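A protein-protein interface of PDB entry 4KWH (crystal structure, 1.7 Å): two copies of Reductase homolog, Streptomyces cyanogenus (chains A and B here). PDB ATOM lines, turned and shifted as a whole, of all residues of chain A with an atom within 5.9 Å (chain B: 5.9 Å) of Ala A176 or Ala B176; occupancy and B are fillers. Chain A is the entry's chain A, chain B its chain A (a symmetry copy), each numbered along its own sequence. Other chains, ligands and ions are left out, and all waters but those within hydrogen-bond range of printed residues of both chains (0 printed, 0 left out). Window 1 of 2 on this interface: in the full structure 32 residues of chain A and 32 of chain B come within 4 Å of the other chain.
Met B128 touches Met A128 (CG to CG, 3.7 Å). Met B172 touches Ala A132. Met A172 touches Ala B132 (CE to O, 3.6 Å). CA of Met A172 touches CB of Gln B179, 3.8 Å away. Met A172 touches Ile B180. Met B172 touches Ala A176 (O to CB, 3.4 Å). N of Ala A176 touches N of Ala B176, at 3.96 Å. Gln A179 touches Gly B171 (CG to O, 3.3 Å). Gln A179 touches Met B172. Ile A180 touches Met B172.
Of chain B, only Met B172 (3.4 Å) and Ala B176 (3.96 Å) come within 4 Å of Ala A176. Printed residues of chain A within 4 Å of Ala B176: Met A172 (3.4 Å) and Ala A176 (3.96 Å). Printed residues of chain A within 4 Å of Gly B171: Gln A179. Printed residues of chain B within 4 Å of Gly A171: Gln B179. Of the printed residues of chain A, Gln B179 touches Gly A171 and Met A172. Of the printed residues of chain B, Gln A179 touches Gly B171 (3.3 Å) and Met B172 (3.8 Å). Printed residues of chain B within 4 Å of Met A172: Ala B132 (3.6 Å), Ala B176 (3.4 Å), Gln B179 (3.8 Å) and Ile B180 (3.9 Å). Gly B175 touches none of the printed residues of chain A. Glu A178 touches none of the printed residues of chain B. The nearest residue of chain B that does not touch Ala A176 is Met B128 (4.1 Å). The nearest printed residue of chain A that does not touch Met B128 is Ala A176 (4.1 Å).
Printed residues of chain B that touch a printed residue of chain A: Met B128, Ala B132, Gly B171, Met B172, Ala B176, Gln B179 and Ile B180. Printed residues of chain A that touch a printed residue of chain B: Met A128, Ala A132, Gly A171, Met A172, Ala A176, Gln A179 and Ile A180. Among the printed residues, no Asp or Glu carboxylate lies within 4 Å of a Lys or Arg side-chain nitrogen of the other chain.
Ala A132 touches Met B172, and with the chains exchanged Met A172 touches Ala B132. Met A172 touches Ala B176, and with the chains exchanged Ala A176 touches Met B172. Met A172 touches Ile B180, and with the chains exchanged Ile A180 touches Met B172. Ala B176 touches its own counterpart, Ala A176. Of the 12 pairs that touch across the chains among the printed residues, 12 have their exchanged pair printed and touching as well.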
ATOM      1  N   MET A 128      33.943 -19.321  -6.036  1.00  0.00           N
ATOM      2  CA  MET A 128      33.680 -18.571  -7.252  1.00  0.00           C
ATOM      3  C   MET A 128      34.895 -18.560  -8.187  1.00  0.00           C
ATOM      4  O   MET A 128      34.719 -18.643  -9.406  1.00  0.00           O
ATOM      5  CB  MET A 128      33.268 -17.158  -6.900  1.00  0.00           C
ATOM      6  CG  MET A 128      32.541 -16.410  -7.991  1.00  0.00           C
ATOM      7  SD  MET A 128      31.006 -17.237  -8.499  1.00  0.00           S
ATOM      8  CE  MET A 128      29.807 -16.890  -7.221  1.00  0.00           C
ATOM      9  N   ALA A 132      33.593 -20.736 -11.410  1.00  0.00           N
ATOM     10  CA  ALA A 132      32.963 -19.796 -12.350  1.00  0.00           C
ATOM     11  C   ALA A 132      33.962 -18.905 -13.060  1.00  0.00           C
ATOM     12  O   ALA A 132      33.919 -18.778 -14.279  1.00  0.00           O
ATOM     13  CB  ALA A 132      31.943 -18.940 -11.608  1.00  0.00           C
ATOM     14  N   GLY A 171      26.177 -23.591  -5.097  1.00  0.00           N
ATOM     15  CA  GLY A 171      25.047 -23.309  -5.976  1.00  0.00           C
ATOM     16  C   GLY A 171      25.207 -22.009  -6.724  1.00  0.00           C
ATOM     17  O   GLY A 171      25.025 -21.943  -7.945  1.00  0.00           O
ATOM     18  N   MET A 172      25.551 -20.949  -5.996  1.00  0.00           N
ATOM     19  CA  MET A 172      25.807 -19.654  -6.643  1.00  0.00           C
ATOM     20  C   MET A 172      26.876 -19.748  -7.735  1.00  0.00           C
ATOM     21  O   MET A 172      26.718 -19.158  -8.843  1.00  0.00           O
ATOM     22  CB  MET A 172      26.203 -18.620  -5.588  1.00  0.00           C
ATOM     23  CG  MET A 172      25.075 -18.234  -4.636  1.00  0.00           C
ATOM     24  SD  MET A 172      25.575 -16.966  -3.451  1.00  0.00           S
ATOM     25  CE  MET A 172      25.817 -15.586  -4.587  1.00  0.00           C
ATOM     26  N   SER A 173      27.980 -20.440  -7.422  1.00  0.00           N
ATOM     27  CA  SER A 173      29.071 -20.579  -8.370  1.00  0.00           C
ATOM     28  C   SER A 173      28.637 -21.325  -9.640  1.00  0.00           C
ATOM     29  O   SER A 173      29.018 -20.937 -10.745  1.00  0.00           O
ATOM     30  CB  SER A 173      30.306 -21.213  -7.736  1.00  0.00           C
ATOM     31  OG  SER A 173      30.185 -22.618  -7.537  1.00  0.00           O
ATOM     32  N   LYS A 174      27.823 -22.358  -9.475  1.00  0.00           N
ATOM     33  CA  LYS A 174      27.327 -23.145 -10.604  1.00  0.00           C
ATOM     34  C   LYS A 174      26.239 -22.381 -11.404  1.00  0.00           C
ATOM     35  O   LYS A 174      26.135 -22.529 -12.643  1.00  0.00           O
ATOM     36  CB  LYS A 174      26.841 -24.517 -10.116  1.00  0.00           C
ATOM     37  CG  LYS A 174      27.945 -25.440  -9.596  1.00  0.00           C
ATOM     38  CD  LYS A 174      29.019 -25.714 -10.632  1.00  0.00           C
ATOM     39  CE  LYS A 174      29.873 -26.896 -10.224  1.00  0.00           C
ATOM     40  NZ  LYS A 174      30.848 -27.367 -11.227  1.00  0.00           N
ATOM     41  N   GLY A 175      25.446 -21.550 -10.723  1.00  0.00           N
ATOM     42  CA  GLY A 175      24.511 -20.675 -11.390  1.00  0.00           C
ATOM     43  C   GLY A 175      25.236 -19.695 -12.293  1.00  0.00           C
ATOM     44  O   GLY A 175      24.808 -19.440 -13.429  1.00  0.00           O
ATOM     45  N   ALA A 176      26.360 -19.165 -11.819  1.00  0.00           N
ATOM     46  CA  ALA A 176      27.203 -18.317 -12.679  1.00  0.00           C
ATOM     47  C   ALA A 176      27.751 -19.109 -13.869  1.00  0.00           C
ATOM     48  O   ALA A 176      27.763 -18.633 -15.012  1.00  0.00           O
ATOM     49  CB  ALA A 176      28.349 -17.694 -11.879  1.00  0.00           C
ATOM     50  N   LEU A 177      28.231 -20.306 -13.598  1.00  0.00           N
ATOM     51  CA  LEU A 177      28.830 -21.153 -14.631  1.00  0.00           C
ATOM     52  C   LEU A 177      27.807 -21.409 -15.731  1.00  0.00           C
ATOM     53  O   LEU A 177      28.143 -21.352 -16.913  1.00  0.00           O
ATOM     54  CB  LEU A 177      29.280 -22.485 -14.049  1.00  0.00           C
ATOM     55  CG  LEU A 177      29.871 -23.509 -15.019  1.00  0.00           C
ATOM     56  CD1 LEU A 177      31.250 -23.096 -15.516  1.00  0.00           C
ATOM     57  CD2 LEU A 177      29.918 -24.873 -14.334  1.00  0.00           C
ATOM     58  N   GLU A 178      26.546 -21.654 -15.348  1.00  0.00           N
ATOM     59  CA  GLU A 178      25.519 -21.956 -16.353  1.00  0.00           C
ATOM     60  C   GLU A 178      25.261 -20.821 -17.337  1.00  0.00           C
ATOM     61  O   GLU A 178      24.858 -21.067 -18.461  1.00  0.00           O
ATOM     62  CB  GLU A 178      24.215 -22.424 -15.685  1.00  0.00           C
ATOM     63  CG  GLU A 178      24.370 -23.825 -15.144  1.00  0.00           C
ATOM     64  CD  GLU A 178      23.132 -24.340 -14.434  1.00  0.00           C
ATOM     65  OE1 GLU A 178      22.036 -23.737 -14.584  1.00  0.00           O
ATOM     66  OE2 GLU A 178      23.268 -25.355 -13.717  1.00  0.00           O
ATOM     67  N   GLN A 179      25.506 -19.585 -16.929  1.00  0.00           N
ATOM     68  CA  GLN A 179      25.311 -18.450 -17.822  1.00  0.00           C
ATOM     69  C   GLN A 179      26.315 -18.451 -18.969  1.00  0.00           C
ATOM     70  O   GLN A 179      26.057 -17.837 -20.009  1.00  0.00           O
ATOM     71  CB  GLN A 179      25.403 -17.145 -17.043  1.00  0.00           C
ATOM     72  CG  GLN A 179      24.275 -16.951 -16.038  1.00  0.00           C
ATOM     73  CD  GLN A 179      22.999 -16.549 -16.741  1.00  0.00           C
ATOM     74  OE1 GLN A 179      22.999 -15.601 -17.545  1.00  0.00           O
ATOM     75  NE2 GLN A 179      21.909 -17.302 -16.496  1.00  0.00           N
ATOM     76  N   ILE A 180      27.459 -19.099 -18.791  1.00  0.00           N
ATOM     77  CA  ILE A 180      28.430 -19.143 -19.886  1.00  0.00           C
ATOM     78  C   ILE A 180      27.782 -19.739 -21.151  1.00  0.00           C
ATOM     79  O   ILE A 180      27.896 -19.165 -22.254  1.00  0.00           O
ATOM     80  CB  ILE A 180      29.706 -19.898 -19.484  1.00  0.00           C
ATOM     81  CG1 ILE A 180      30.465 -19.097 -18.417  1.00  0.00           C
ATOM     82  CG2 ILE A 180      30.618 -20.130 -20.702  1.00  0.00           C
ATOM     83  CD1 ILE A 180      31.664 -19.822 -17.816  1.00  0.00           C
ATOM     84  N   MET B 128      31.265  -9.487  -9.934  1.00  0.00           N
ATOM     85  CA  MET B 128      30.870 -10.528  -9.002  1.00  0.00           C
ATOM     86  C   MET B 128      30.838 -10.015  -7.557  1.00  0.00           C
ATOM     87  O   MET B 128      29.946 -10.406  -6.798  1.00  0.00           O
ATOM     88  CB  MET B 128      31.812 -11.707  -9.126  1.00  0.00           C
ATOM     89  CG  MET B 128      31.286 -13.010  -8.574  1.00  0.00           C
ATOM     90  SD  MET B 128      29.752 -13.543  -9.388  1.00  0.00           S
ATOM     91  CE  MET B 128      30.234 -14.207 -10.974  1.00  0.00           C
ATOM     92  N   ALA B 132      26.851 -10.183  -6.612  1.00  0.00           N
ATOM     93  CA  ALA B 132      26.586 -11.520  -6.058  1.00  0.00           C
ATOM     94  C   ALA B 132      27.162 -11.713  -4.669  1.00  0.00           C
ATOM     95  O   ALA B 132      26.464 -12.168  -3.769  1.00  0.00           O
ATOM     96  CB  ALA B 132      27.141 -12.582  -7.000  1.00  0.00           C
ATOM     97  N   GLY B 171      25.636 -11.151 -16.642  1.00  0.00           N
ATOM     98  CA  GLY B 171      24.764 -12.321 -16.625  1.00  0.00           C
ATOM     99  C   GLY B 171      25.203 -13.355 -15.619  1.00  0.00           C
ATOM    100  O   GLY B 171      24.403 -13.857 -14.821  1.00  0.00           O
ATOM    101  N   MET B 172      26.491 -13.692 -15.645  1.00  0.00           N
ATOM    102  CA  MET B 172      27.032 -14.634 -14.654  1.00  0.00           C
ATOM    103  C   MET B 172      26.770 -14.183 -13.215  1.00  0.00           C
ATOM    104  O   MET B 172      26.387 -15.012 -12.339  1.00  0.00           O
ATOM    105  CB  MET B 172      28.530 -14.829 -14.893  1.00  0.00           C
ATOM    106  CG  MET B 172      28.866 -15.565 -16.186  1.00  0.00           C
ATOM    107  SD  MET B 172      30.642 -15.825 -16.391  1.00  0.00           S
ATOM    108  CE  MET B 172      30.927 -16.972 -15.028  1.00  0.00           C
ATOM    109  N   SER B 173      27.015 -12.893 -12.946  1.00  0.00           N
ATOM    110  CA  SER B 173      26.823 -12.355 -11.612  1.00  0.00           C
ATOM    111  C   SER B 173      25.359 -12.451 -11.159  1.00  0.00           C
ATOM    112  O   SER B 173      25.090 -12.790 -10.006  1.00  0.00           O
ATOM    113  CB  SER B 173      27.365 -10.935 -11.481  1.00  0.00           C
ATOM    114  OG  SER B 173      26.533  -9.952 -12.090  1.00  0.00           O
ATOM    115  N   LYS B 174      24.435 -12.188 -12.072  1.00  0.00           N
ATOM    116  CA  LYS B 174      23.005 -12.254 -11.773  1.00  0.00           C
ATOM    117  C   LYS B 174      22.509 -13.719 -11.654  1.00  0.00           C
ATOM    118  O   LYS B 174      21.596 -14.022 -10.853  1.00  0.00           O
ATOM    119  CB  LYS B 174      22.211 -11.449 -12.812  1.00  0.00           C
ATOM    120  CG  LYS B 174      22.438  -9.937 -12.759  1.00  0.00           C
ATOM    121  CD  LYS B 174      22.097  -9.338 -11.407  1.00  0.00           C
ATOM    122  CE  LYS B 174      21.975  -7.831 -11.500  1.00  0.00           C
ATOM    123  NZ  LYS B 174      21.485  -7.145 -10.288  1.00  0.00           N
ATOM    124  N   GLY B 175      23.112 -14.635 -12.418  1.00  0.00           N
ATOM    125  CA  GLY B 175      22.839 -16.045 -12.271  1.00  0.00           C
ATOM    126  C   GLY B 175      23.229 -16.531 -10.888  1.00  0.00           C
ATOM    127  O   GLY B 175      22.493 -17.302 -10.253  1.00  0.00           O
ATOM    128  N   ALA B 176      24.367 -16.059 -10.387  1.00  0.00           N
ATOM    129  CA  ALA B 176      24.753 -16.363  -8.999  1.00  0.00           C
ATOM    130  C   ALA B 176      23.748 -15.773  -8.005  1.00  0.00           C
ATOM    131  O   ALA B 176      23.346 -16.422  -7.030  1.00  0.00           O
ATOM    132  CB  ALA B 176      26.163 -15.854  -8.697  1.00  0.00           C
ATOM    133  N   LEU B 177      23.364 -14.533  -8.235  1.00  0.00           N
ATOM    134  CA  LEU B 177      22.444 -13.829  -7.339  1.00  0.00           C
ATOM    135  C   LEU B 177      21.137 -14.605  -7.243  1.00  0.00           C
ATOM    136  O   LEU B 177      20.587 -14.757  -6.153  1.00  0.00           O
ATOM    137  CB  LEU B 177      22.155 -12.425  -7.853  1.00  0.00           C
ATOM    138  CG  LEU B 177      21.158 -11.582  -7.058  1.00  0.00           C
ATOM    139  CD1 LEU B 177      21.730 -11.130  -5.720  1.00  0.00           C
ATOM    140  CD2 LEU B 177      20.731 -10.386  -7.906  1.00  0.00           C
ATOM    141  N   GLU B 178      20.654 -15.133  -8.377  1.00  0.00           N
ATOM    142  CA  GLU B 178      19.375 -15.852  -8.366  1.00  0.00           C
ATOM    143  C   GLU B 178      19.374 -17.102  -7.493  1.00  0.00           C
ATOM    144  O   GLU B 178      18.336 -17.495  -6.990  1.00  0.00           O
ATOM    145  CB  GLU B 178      18.908 -16.169  -9.796  1.00  0.00           C
ATOM    146  CG  GLU B 178      18.416 -14.918 -10.482  1.00  0.00           C
ATOM    147  CD  GLU B 178      17.974 -15.147 -11.915  1.00  0.00           C
ATOM    148  OE1 GLU B 178      17.778 -16.323 -12.323  1.00  0.00           O
ATOM    149  OE2 GLU B 178      17.831 -14.134 -12.635  1.00  0.00           O
ATOM    150  N   GLN B 179      20.531 -17.717  -7.297  1.00  0.00           N
ATOM    151  CA  GLN B 179      20.614 -18.901  -6.452  1.00  0.00           C
ATOM    152  C   GLN B 179      20.348 -18.573  -4.988  1.00  0.00           C
ATOM    153  O   GLN B 179      19.978 -19.466  -4.218  1.00  0.00           O
ATOM    154  CB  GLN B 179      21.979 -19.561  -6.604  1.00  0.00           C
ATOM    155  CG  GLN B 179      22.224 -20.146  -7.989  1.00  0.00           C
ATOM    156  CD  GLN B 179      21.473 -21.446  -8.159  1.00  0.00           C
ATOM    157  OE1 GLN B 179      21.580 -22.347  -7.309  1.00  0.00           O
ATOM    158  NE2 GLN B 179      20.656 -21.538  -9.225  1.00  0.00           N
ATOM    159  N   ILE B 180      20.556 -17.327  -4.583  1.00  0.00           N
ATOM    160  CA  ILE B 180      20.279 -16.975  -3.190  1.00  0.00           C
ATOM    161  C   ILE B 180      18.819 -17.313  -2.832  1.00  0.00           C
ATOM    162  O   ILE B 180      18.550 -17.956  -1.796  1.00  0.00           O
ATOM    163  CB  ILE B 180      20.617 -15.505  -2.897  1.00  0.00           C
ATOM    164  CG1 ILE B 180      22.135 -15.297  -2.983  1.00  0.00           C
ATOM    165  CG2 ILE B 180      20.116 -15.091  -1.501  1.00  0.00           C
ATOM    166  CD1 ILE B 180      22.581 -13.843  -2.876  1.00  0.00           C
